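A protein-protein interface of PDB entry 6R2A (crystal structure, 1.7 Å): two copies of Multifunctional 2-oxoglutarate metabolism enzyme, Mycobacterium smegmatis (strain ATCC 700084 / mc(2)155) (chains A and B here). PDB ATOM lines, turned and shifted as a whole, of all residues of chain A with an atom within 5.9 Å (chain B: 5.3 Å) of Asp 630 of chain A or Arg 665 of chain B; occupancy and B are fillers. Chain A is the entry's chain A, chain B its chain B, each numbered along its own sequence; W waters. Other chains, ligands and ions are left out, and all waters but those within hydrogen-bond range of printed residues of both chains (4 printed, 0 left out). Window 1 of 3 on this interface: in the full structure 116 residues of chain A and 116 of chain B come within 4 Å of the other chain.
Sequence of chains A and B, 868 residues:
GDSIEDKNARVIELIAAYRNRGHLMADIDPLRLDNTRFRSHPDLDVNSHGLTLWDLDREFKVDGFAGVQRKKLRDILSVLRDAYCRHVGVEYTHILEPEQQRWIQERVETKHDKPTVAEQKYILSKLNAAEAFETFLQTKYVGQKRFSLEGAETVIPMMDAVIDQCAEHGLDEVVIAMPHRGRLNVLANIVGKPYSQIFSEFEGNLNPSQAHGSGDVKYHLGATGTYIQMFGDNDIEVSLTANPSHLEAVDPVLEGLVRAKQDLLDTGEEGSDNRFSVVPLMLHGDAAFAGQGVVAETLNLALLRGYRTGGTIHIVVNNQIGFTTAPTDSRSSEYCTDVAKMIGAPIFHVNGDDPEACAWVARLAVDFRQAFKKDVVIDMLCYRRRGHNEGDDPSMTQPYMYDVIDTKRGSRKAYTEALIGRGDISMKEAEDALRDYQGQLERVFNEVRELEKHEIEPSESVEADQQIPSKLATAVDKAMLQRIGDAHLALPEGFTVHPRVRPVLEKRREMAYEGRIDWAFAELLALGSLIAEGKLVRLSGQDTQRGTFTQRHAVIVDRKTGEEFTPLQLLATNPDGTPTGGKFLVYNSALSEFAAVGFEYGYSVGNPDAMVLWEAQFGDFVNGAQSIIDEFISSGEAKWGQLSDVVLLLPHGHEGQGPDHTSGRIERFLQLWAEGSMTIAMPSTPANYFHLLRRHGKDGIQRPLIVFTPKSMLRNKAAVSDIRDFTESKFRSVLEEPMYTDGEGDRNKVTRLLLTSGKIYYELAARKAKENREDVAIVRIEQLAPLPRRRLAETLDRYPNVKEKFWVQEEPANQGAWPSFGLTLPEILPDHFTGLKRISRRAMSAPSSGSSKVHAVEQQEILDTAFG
The side-chain carboxylate of Asp 630 of chain A is in hydrogen-bond range of the side-chain amide nitrogen of Asn 623 of chain B.
OD2 of Asp 630 of chain A lies within salt-bridge range of NE of Arg 665 of chain B, at 3.6 Å.
The guanidinium group (NH1) of Arg 668 of chain B is in salt-bridge range of the side-chain carboxylate (OD2) of Asp 630 of chain A.
The side-chain carboxylate (OE2) of Glu 631 of chain A lies within hydrogen-bond range of the side-chain amide nitrogen (ND2) of Asn 623 of chain B.
The side-chain carboxylate (OE2) of Glu 631 of chain A is in salt-bridge range of the guanidinium group (NH1) of Arg 665 of chain B, 3.95 Å away.
NE2 of Gln 626 of chain A is in hydrogen-bond range of OD1 of Asp 630 of chain A (2.9 Å).
The side-chain amide oxygen (OE1) of Gln 626 of chain A sits at hydrogen-bond distance from the guanidinium group (NH1) of Arg 668 of chain A.
O of Ile 629 of chain A sits at hydrogen-bond distance from N of Ser 634 of chain A (2.9 Å).
O of Asp 630 of chain A sits at hydrogen-bond distance from OG of Ser 634 of chain A.
The guanidinium group of Arg 668 of chain B is in hydrogen-bond range of the side-chain amide oxygen of Gln 626 of chain B.
The backbone NH (N) of Arg 665 of chain B sits at hydrogen-bond distance from the side-chain hydroxyl (OG) of Ser 663 of chain B (2.9 Å).
Among the printed residues, merely in contact across the chains: Gln 626 of chain A with Asn 623 of chain B, Gln 626 of chain A with Gln 626 of chain B, Gln 626 of chain A with Arg 668 of chain B, Ser 627 of chain A with Asn 623 of chain B, Ser 634 of chain A with Ser 845 of chain B, Ser 635 of chain A with Ser 845 of chain B, Arg 668 of chain A with Gln 626 of chain B, Arg 668 of chain A with Arg 668 of chain B, Leu 672 of chain A with Arg 665 of chain B and Leu 672 of chain A with Arg 668 of chain B.
Asp 630 of chain A touches three residues of chain B.
Of the printed residues of chain B, Ser 635 of chain A touches Ser 845.
Printed residues of chain B within 4 Å of Arg 668 of chain A: Gln 626 (3.3 Å) and Arg 668 (3.5 Å).
Arg 665 of chain B touches just these residues of chain A: Asp 630 (3.6 Å), Glu 631 (3.95 Å) and Leu 672 (3.5 Å).
Printed residues of chain A within 4 Å of Arg 668 of chain B: Gln 626, Asp 630, Arg 668 and Leu 672.
Phe 669 of chain B touches none of the printed residues of chain A.
Printed residues of chain A within 4 Å of Ser 845 of chain B: Ser 634 and Ser 635.
Pro 847 of chain B touches none of the printed residues of chain A.
The nearest residue of chain B that does not touch Asp 630 of chain A is Gln 626 of chain B (5.0 Å).
The nearest printed residue of chain B that does not touch Ser 635 of chain A is Pro 847 of chain B (6.0 Å).
Hydrophobic or aromatic side chains of chain A that line the printed part of chain B: Leu 672.
Of the 13 printed residues of chain B, 5 touch a printed residue of chain A.
Among the printed residues, 15 pairs touch across the chains.
Among the printed residues, Asp or Glu carboxylates within 4 Å of a Lys or Arg side-chain nitrogen of the other chain: Asp 630 of chain A with Arg 665 of chain B (3.6 Å), Asp 630 of chain A with Arg 668 of chain B (2.8 Å) and Glu 631 of chain A with Arg 665 of chain B (3.95 Å).
Gln 626 of chain B touches its own counterpart, Gln 626 of chain A.
Gln 626 of chain A touches Arg 668 of chain B, and with the chains exchanged Arg 668 of chain A touches Gln 626 of chain B.
Arg 668 of chain B touches its own counterpart, Arg 668 of chain A.
2 positions are printed for both chains.
Water W1 lies within hydrogen-bond range of O of Leu 672 of chain A, O of Ser 634 of chain A and OG of Ser 845 of chain B.
Water W3 bridges OE2 of Glu 631 of chain A (2.8 Å) and NH1 of Arg 665 of chain B (3.0 Å).
Water W2 bridges O of Leu 672 of chain A and O of Ser 845 of chain B.
Water W4 lies within hydrogen-bond range of O of Asp 630 of chain A (2.9 Å), O of Ser 845 of chain B (2.9 Å) and NH1 of Arg 665 of chain B (3.0 Å).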
ATOM      1  N   ALA A 625      -7.699 -16.024  20.794  1.00  0.00           N
ATOM      2  CA  ALA A 625      -7.548 -16.962  19.667  1.00  0.00           C
ATOM      3  C   ALA A 625      -6.073 -17.205  19.363  1.00  0.00           C
ATOM      4  O   ALA A 625      -5.720 -17.561  18.226  1.00  0.00           O
ATOM      5  CB  ALA A 625      -8.260 -16.410  18.429  1.00  0.00           C
ATOM      6  N   GLN A 626      -5.198 -17.008  20.378  1.00  0.00           N
ATOM      7  CA  GLN A 626      -3.750 -17.114  20.136  1.00  0.00           C
ATOM      8  C   GLN A 626      -3.344 -18.459  19.533  1.00  0.00           C
ATOM      9  O   GLN A 626      -2.468 -18.458  18.656  1.00  0.00           O
ATOM     10  CB  GLN A 626      -2.922 -16.835  21.410  1.00  0.00           C
ATOM     11  CG  GLN A 626      -1.447 -16.492  21.078  1.00  0.00           C
ATOM     12  CD  GLN A 626      -1.366 -15.148  20.365  1.00  0.00           C
ATOM     13  OE1 GLN A 626      -1.851 -14.135  20.883  1.00  0.00           O
ATOM     14  NE2 GLN A 626      -0.772 -15.110  19.155  1.00  0.00           N
ATOM     15  N   SER A 627      -3.963 -19.586  19.989  1.00  0.00           N
ATOM     16  CA  SER A 627      -3.595 -20.905  19.444  1.00  0.00           C
ATOM     17  C   SER A 627      -3.890 -20.960  17.937  1.00  0.00           C
ATOM     18  O   SER A 627      -3.080 -21.492  17.181  1.00  0.00           O
ATOM     19  CB  SER A 627      -4.355 -22.022  20.165  1.00  0.00           C
ATOM     20  OG  SER A 627      -4.077 -21.983  21.557  1.00  0.00           O
ATOM     21  N   ILE A 628      -5.014 -20.361  17.483  1.00  0.00           N
ATOM     22  CA  ILE A 628      -5.314 -20.374  16.031  1.00  0.00           C
ATOM     23  C   ILE A 628      -4.305 -19.497  15.274  1.00  0.00           C
ATOM     24  O   ILE A 628      -3.823 -19.896  14.221  1.00  0.00           O
ATOM     25  CB  ILE A 628      -6.774 -19.928  15.748  1.00  0.00           C
ATOM     26  CG1 ILE A 628      -7.792 -20.887  16.469  1.00  0.00           C
ATOM     27  CG2 ILE A 628      -7.040 -19.871  14.211  1.00  0.00           C
ATOM     28  CD1 ILE A 628      -7.728 -22.411  16.027  1.00  0.00           C
ATOM     29  N   ILE A 629      -4.012 -18.304  15.792  1.00  0.00           N
ATOM     30  CA  ILE A 629      -3.034 -17.413  15.155  1.00  0.00           C
ATOM     31  C   ILE A 629      -1.673 -18.113  15.039  1.00  0.00           C
ATOM     32  O   ILE A 629      -1.072 -18.129  13.948  1.00  0.00           O
ATOM     33  CB  ILE A 629      -2.925 -16.080  15.940  1.00  0.00           C
ATOM     34  CG1 ILE A 629      -4.226 -15.246  15.800  1.00  0.00           C
ATOM     35  CG2 ILE A 629      -1.666 -15.260  15.480  1.00  0.00           C
ATOM     36  CD1 ILE A 629      -4.363 -14.175  16.904  1.00  0.00           C
ATOM     37  N   ASP A 630      -1.180 -18.656  16.154  1.00  0.00           N
ATOM     38  CA  ASP A 630       0.139 -19.273  16.166  1.00  0.00           C
ATOM     39  C   ASP A 630       0.236 -20.545  15.332  1.00  0.00           C
ATOM     40  O   ASP A 630       1.243 -20.751  14.647  1.00  0.00           O
ATOM     41  CB  ASP A 630       0.556 -19.633  17.606  1.00  0.00           C
ATOM     42  CG  ASP A 630       0.746 -18.461  18.561  1.00  0.00           C
ATOM     43  OD1 ASP A 630       0.767 -17.289  18.083  1.00  0.00           O
ATOM     44  OD2 ASP A 630       0.937 -18.715  19.771  1.00  0.00           O
ATOM     45  N   GLU A 631      -0.766 -21.430  15.460  1.00  0.00           N
ATOM     46  CA  GLU A 631      -0.703 -22.784  14.901  1.00  0.00           C
ATOM     47  C   GLU A 631      -1.296 -22.945  13.497  1.00  0.00           C
ATOM     48  O   GLU A 631      -0.986 -23.934  12.839  1.00  0.00           O
ATOM     49  CB  GLU A 631      -1.400 -23.766  15.853  1.00  0.00           C
ATOM     50  CG  GLU A 631      -0.803 -23.791  17.263  1.00  0.00           C
ATOM     51  CD  GLU A 631       0.651 -24.211  17.308  1.00  0.00           C
ATOM     52  OE1 GLU A 631       1.017 -25.145  16.549  1.00  0.00           O
ATOM     53  OE2 GLU A 631       1.420 -23.612  18.098  1.00  0.00           O
ATOM     54  N   PHE A 632      -2.198 -22.043  13.078  1.00  0.00           N
ATOM     55  CA  PHE A 632      -2.820 -22.169  11.764  1.00  0.00           C
ATOM     56  C   PHE A 632      -2.527 -20.948  10.879  1.00  0.00           C
ATOM     57  O   PHE A 632      -1.940 -21.078   9.799  1.00  0.00           O
ATOM     58  CB  PHE A 632      -4.356 -22.314  11.926  1.00  0.00           C
ATOM     59  CG  PHE A 632      -4.811 -23.657  12.447  1.00  0.00           C
ATOM     60  CD1 PHE A 632      -5.065 -24.714  11.573  1.00  0.00           C
ATOM     61  CD2 PHE A 632      -5.079 -23.839  13.803  1.00  0.00           C
ATOM     62  CE1 PHE A 632      -5.515 -25.952  12.056  1.00  0.00           C
ATOM     63  CE2 PHE A 632      -5.544 -25.080  14.287  1.00  0.00           C
ATOM     64  CZ  PHE A 632      -5.787 -26.111  13.401  1.00  0.00           C
ATOM     65  N   ILE A 633      -2.964 -19.768  11.313  1.00  0.00           N
ATOM     66  CA  ILE A 633      -2.873 -18.558  10.480  1.00  0.00           C
ATOM     67  C   ILE A 633      -1.432 -18.207  10.114  1.00  0.00           C
ATOM     68  O   ILE A 633      -1.113 -18.069   8.921  1.00  0.00           O
ATOM     69  CB  ILE A 633      -3.593 -17.360  11.182  1.00  0.00           C
ATOM     70  CG1 ILE A 633      -5.142 -17.595  11.167  1.00  0.00           C
ATOM     71  CG2 ILE A 633      -3.248 -16.006  10.511  1.00  0.00           C
ATOM     72  CD1 ILE A 633      -5.954 -16.571  12.025  1.00  0.00           C
ATOM     73  N   SER A 634      -0.558 -18.062  11.140  1.00  0.00           N
ATOM     74  CA  SER A 634       0.804 -17.592  10.863  1.00  0.00           C
ATOM     75  C   SER A 634       1.727 -18.648  10.252  1.00  0.00           C
ATOM     76  O   SER A 634       2.782 -18.289   9.729  1.00  0.00           O
ATOM     77  CB  SER A 634       1.454 -17.100  12.165  1.00  0.00           C
ATOM     78  OG  SER A 634       1.675 -18.184  13.057  1.00  0.00           O
ATOM     79  N   SER A 635       1.352 -19.936  10.333  1.00  0.00           N
ATOM     80  CA  SER A 635       2.301 -21.006  10.039  1.00  0.00           C
ATOM     81  C   SER A 635       1.798 -22.187   9.190  1.00  0.00           C
ATOM     82  O   SER A 635       2.626 -23.042   8.841  1.00  0.00           O
ATOM     83  CB  SER A 635       2.791 -21.562  11.379  1.00  0.00           C
ATOM     84  OG  SER A 635       1.696 -21.971  12.193  1.00  0.00           O
ATOM     85  N   LYS A 639       4.114 -25.126   7.312  1.00  0.00           N
ATOM     86  CA  LYS A 639       4.093 -26.460   7.932  1.00  0.00           C
ATOM     87  C   LYS A 639       3.422 -27.522   7.067  1.00  0.00           C
ATOM     88  O   LYS A 639       3.865 -28.677   7.081  1.00  0.00           O
ATOM     89  CB  LYS A 639       3.370 -26.419   9.295  1.00  0.00           C
ATOM     90  CG  LYS A 639       4.099 -25.584  10.373  1.00  0.00           C
ATOM     91  CD  LYS A 639       3.463 -25.694  11.770  1.00  0.00           C
ATOM     92  CE  LYS A 639       2.019 -25.192  11.804  1.00  0.00           C
ATOM     93  NZ  LYS A 639       1.529 -25.089  13.209  1.00  0.00           N
ATOM     94  N   ARG A 668       3.260  -8.403  18.342  1.00  0.00           N
ATOM     95  CA  ARG A 668       3.171  -9.865  18.337  1.00  0.00           C
ATOM     96  C   ARG A 668       3.007 -10.388  16.902  1.00  0.00           C
ATOM     97  O   ARG A 668       3.675 -11.365  16.527  1.00  0.00           O
ATOM     98  CB  ARG A 668       2.019 -10.348  19.247  1.00  0.00           C
ATOM     99  CG  ARG A 668       2.000 -11.876  19.424  1.00  0.00           C
ATOM    100  CD  ARG A 668       1.030 -12.283  20.534  1.00  0.00           C
ATOM    101  NE  ARG A 668       1.479 -11.782  21.846  1.00  0.00           N
ATOM    102  CZ  ARG A 668       0.717 -11.765  22.934  1.00  0.00           C
ATOM    103  NH1 ARG A 668      -0.524 -12.245  22.894  1.00  0.00           N
ATOM    104  NH2 ARG A 668       1.205 -11.312  24.088  1.00  0.00           N
ATOM    105  N   LEU A 672       5.652 -12.751  14.845  1.00  0.00           N
ATOM    106  CA  LEU A 672       5.220 -14.007  14.219  1.00  0.00           C
ATOM    107  C   LEU A 672       5.541 -14.025  12.730  1.00  0.00           C
ATOM    108  O   LEU A 672       5.787 -15.085  12.164  1.00  0.00           O
ATOM    109  CB  LEU A 672       3.704 -14.187  14.393  1.00  0.00           C
ATOM    110  CG  LEU A 672       3.287 -14.720  15.770  1.00  0.00           C
ATOM    111  CD1 LEU A 672       1.790 -14.499  15.980  1.00  0.00           C
ATOM    112  CD2 LEU A 672       3.630 -16.227  15.903  1.00  0.00           C
ATOM    113  N   ASN B 623       0.674 -21.144  24.841  1.00  0.00           N
ATOM    114  CA  ASN B 623      -0.132 -20.162  24.095  1.00  0.00           C
ATOM    115  C   ASN B 623      -1.666 -20.418  24.265  1.00  0.00           C
ATOM    116  O   ASN B 623      -2.457 -19.492  24.081  1.00  0.00           O
ATOM    117  CB  ASN B 623       0.243 -20.130  22.617  1.00  0.00           C
ATOM    118  CG  ASN B 623       0.231 -21.460  21.913  1.00  0.00           C
ATOM    119  OD1 ASN B 623      -0.033 -22.542  22.515  1.00  0.00           O
ATOM    120  ND2 ASN B 623       0.504 -21.415  20.604  1.00  0.00           N
ATOM    121  N   GLN B 626      -2.793 -17.846  26.679  1.00  0.00           N
ATOM    122  CA  GLN B 626      -2.313 -16.501  26.349  1.00  0.00           C
ATOM    123  C   GLN B 626      -3.101 -15.393  27.059  1.00  0.00           C
ATOM    124  O   GLN B 626      -2.476 -14.406  27.477  1.00  0.00           O
ATOM    125  CB  GLN B 626      -2.304 -16.249  24.825  1.00  0.00           C
ATOM    126  CG  GLN B 626      -1.380 -15.051  24.451  1.00  0.00           C
ATOM    127  CD  GLN B 626       0.077 -15.407  24.703  1.00  0.00           C
ATOM    128  OE1 GLN B 626       0.589 -16.403  24.186  1.00  0.00           O
ATOM    129  NE2 GLN B 626       0.773 -14.607  25.521  1.00  0.00           N
ATOM    130  N   HIS B 652      11.588 -26.529  26.793  1.00  0.00           N
ATOM    131  CA  HIS B 652      11.995 -25.801  25.599  1.00  0.00           C
ATOM    132  C   HIS B 652      13.323 -26.303  25.065  1.00  0.00           C
ATOM    133  O   HIS B 652      14.231 -26.575  25.856  1.00  0.00           O
ATOM    134  CB  HIS B 652      12.170 -24.317  26.051  1.00  0.00           C
ATOM    135  CG  HIS B 652      12.648 -23.389  24.979  1.00  0.00           C
ATOM    136  ND1 HIS B 652      11.760 -22.646  24.230  1.00  0.00           N
ATOM    137  CD2 HIS B 652      13.908 -23.155  24.536  1.00  0.00           C
ATOM    138  CE1 HIS B 652      12.496 -21.978  23.355  1.00  0.00           C
ATOM    139  NE2 HIS B 652      13.803 -22.260  23.499  1.00  0.00           N
ATOM    140  N   SER B 663       9.497 -25.027  21.224  1.00  0.00           N
ATOM    141  CA  SER B 663       9.612 -23.679  21.771  1.00  0.00           C
ATOM    142  C   SER B 663       8.492 -23.214  22.698  1.00  0.00           C
ATOM    143  O   SER B 663       7.310 -23.332  22.375  1.00  0.00           O
ATOM    144  CB  SER B 663       9.676 -22.695  20.601  1.00  0.00           C
ATOM    145  OG  SER B 663       9.722 -21.342  21.037  1.00  0.00           O
ATOM    146  N   GLY B 664       8.904 -22.578  23.798  1.00  0.00           N
ATOM    147  CA  GLY B 664       8.002 -21.906  24.732  1.00  0.00           C
ATOM    148  C   GLY B 664       7.792 -20.441  24.367  1.00  0.00           C
ATOM    149  O   GLY B 664       7.173 -19.691  25.130  1.00  0.00           O
ATOM    150  N   ARG B 665       8.334 -20.020  23.204  1.00  0.00           N
ATOM    151  CA  ARG B 665       8.251 -18.641  22.650  1.00  0.00           C
ATOM    152  C   ARG B 665       8.860 -17.616  23.628  1.00  0.00           C
ATOM    153  O   ARG B 665       8.192 -16.676  24.106  1.00  0.00           O
ATOM    154  CB  ARG B 665       6.795 -18.246  22.240  1.00  0.00           C
ATOM    155  CG  ARG B 665       6.250 -19.162  21.129  1.00  0.00           C
ATOM    156  CD  ARG B 665       4.874 -18.776  20.583  1.00  0.00           C
ATOM    157  NE  ARG B 665       4.412 -19.812  19.649  1.00  0.00           N
ATOM    158  CZ  ARG B 665       4.588 -19.797  18.328  1.00  0.00           C
ATOM    159  NH1 ARG B 665       4.158 -20.811  17.583  1.00  0.00           N
ATOM    160  NH2 ARG B 665       5.207 -18.779  17.742  1.00  0.00           N
ATOM    161  N   ILE B 666      10.157 -17.786  23.881  1.00  0.00           N
ATOM    162  CA  ILE B 666      10.965 -16.870  24.713  1.00  0.00           C
ATOM    163  C   ILE B 666      10.718 -15.426  24.261  1.00  0.00           C
ATOM    164  O   ILE B 666      10.538 -14.524  25.097  1.00  0.00           O
ATOM    165  CB  ILE B 666      12.472 -17.239  24.548  1.00  0.00           C
ATOM    166  CG1 ILE B 666      12.781 -18.654  25.103  1.00  0.00           C
ATOM    167  CG2 ILE B 666      13.380 -16.157  25.162  1.00  0.00           C
ATOM    168  CD1 ILE B 666      14.219 -19.158  24.670  1.00  0.00           C
ATOM    169  N   GLU B 667      10.731 -15.212  22.928  1.00  0.00           N
ATOM    170  CA  GLU B 667      10.586 -13.886  22.312  1.00  0.00           C
ATOM    171  C   GLU B 667       9.288 -13.187  22.761  1.00  0.00           C
ATOM    172  O   GLU B 667       9.288 -11.968  22.932  1.00  0.00           O
ATOM    173  CB  GLU B 667      10.660 -13.977  20.767  1.00  0.00           C
ATOM    174  CG  GLU B 667       9.597 -14.845  20.091  1.00  0.00           C
ATOM    175  CD  GLU B 667       9.708 -16.359  20.178  1.00  0.00           C
ATOM    176  OE1 GLU B 667      10.733 -16.889  20.676  1.00  0.00           O
ATOM    177  OE2 GLU B 667       8.754 -17.019  19.720  1.00  0.00           O
ATOM    178  N   ARG B 668       8.195 -13.956  22.956  1.00  0.00           N
ATOM    179  CA  ARG B 668       6.910 -13.372  23.359  1.00  0.00           C
ATOM    180  C   ARG B 668       6.969 -12.913  24.818  1.00  0.00           C
ATOM    181  O   ARG B 668       6.494 -11.810  25.130  1.00  0.00           O
ATOM    182  CB  ARG B 668       5.762 -14.375  23.131  1.00  0.00           C
ATOM    183  CG  ARG B 668       4.378 -13.746  23.367  1.00  0.00           C
ATOM    184  CD  ARG B 668       3.252 -14.669  22.878  1.00  0.00           C
ATOM    185  NE  ARG B 668       3.327 -14.846  21.420  1.00  0.00           N
ATOM    186  CZ  ARG B 668       2.666 -15.788  20.748  1.00  0.00           C
ATOM    187  NH1 ARG B 668       1.843 -16.622  21.390  1.00  0.00           N
ATOM    188  NH2 ARG B 668       2.781 -15.873  19.424  1.00  0.00           N
ATOM    189  N   PHE B 669       7.544 -13.750  25.716  1.00  0.00           N
ATOM    190  CA  PHE B 669       7.664 -13.347  27.128  1.00  0.00           C
ATOM    191  C   PHE B 669       8.607 -12.140  27.277  1.00  0.00           C
ATOM    192  O   PHE B 669       8.319 -11.233  28.072  1.00  0.00           O
ATOM    193  CB  PHE B 669       8.147 -14.516  28.003  1.00  0.00           C
ATOM    194  CG  PHE B 669       7.073 -15.551  28.213  1.00  0.00           C
ATOM    195  CD1 PHE B 669       6.116 -15.392  29.215  1.00  0.00           C
ATOM    196  CD2 PHE B 669       6.973 -16.657  27.366  1.00  0.00           C
ATOM    197  CE1 PHE B 669       5.108 -16.360  29.409  1.00  0.00           C
ATOM    198  CE2 PHE B 669       5.963 -17.617  27.552  1.00  0.00           C
ATOM    199  CZ  PHE B 669       5.035 -17.455  28.573  1.00  0.00           C
ATOM    200  N   PHE B 708      12.412 -21.450  31.239  1.00  0.00           N
ATOM    201  CA  PHE B 708      12.530 -22.319  30.072  1.00  0.00           C
ATOM    202  C   PHE B 708      13.381 -23.494  30.534  1.00  0.00           C
ATOM    203  O   PHE B 708      14.554 -23.325  30.905  1.00  0.00           O
ATOM    204  CB  PHE B 708      13.102 -21.560  28.856  1.00  0.00           C
ATOM    205  CG  PHE B 708      12.124 -20.482  28.451  1.00  0.00           C
ATOM    206  CD1 PHE B 708      11.030 -20.783  27.647  1.00  0.00           C
ATOM    207  CD2 PHE B 708      12.243 -19.183  28.952  1.00  0.00           C
ATOM    208  CE1 PHE B 708      10.072 -19.805  27.337  1.00  0.00           C
ATOM    209  CE2 PHE B 708      11.284 -18.202  28.644  1.00  0.00           C
ATOM    210  CZ  PHE B 708      10.211 -18.520  27.836  1.00  0.00           C
ATOM    211  N   SER B 845       8.354 -19.033  10.056  1.00  0.00           N
ATOM    212  CA  SER B 845       6.939 -18.856  10.412  1.00  0.00           C
ATOM    213  C   SER B 845       6.574 -19.802  11.552  1.00  0.00           C
ATOM    214  O   SER B 845       5.792 -19.438  12.437  1.00  0.00           O
ATOM    215  CB  SER B 845       6.039 -19.105   9.206  1.00  0.00           C
ATOM    216  OG  SER B 845       6.283 -18.075   8.263  1.00  0.00           O
ATOM    217  N   PRO B 847       8.102 -22.527  14.768  1.00  0.00           N
ATOM    218  CA  PRO B 847       9.295 -22.513  15.653  1.00  0.00           C
ATOM    219  C   PRO B 847      10.448 -23.417  15.191  1.00  0.00           C
ATOM    220  O   PRO B 847      11.575 -23.231  15.658  1.00  0.00           O
ATOM    221  CB  PRO B 847       8.738 -23.018  16.985  1.00  0.00           C
ATOM    222  CG  PRO B 847       7.252 -22.580  16.935  1.00  0.00           C
ATOM    223  CD  PRO B 847       6.912 -22.987  15.508  1.00  0.00           C
HETATM  224  O   HOH W   1       4.709 -16.214   9.897  1.00  0.00           O
HETATM  225  O   HOH W   2       6.987 -17.113  13.695  1.00  0.00           O
HETATM  226  O   HOH W   3       4.069 -23.808  17.301  1.00  0.00           O
HETATM  227  O   HOH W   4       4.088 -20.325  14.601  1.00  0.00           O
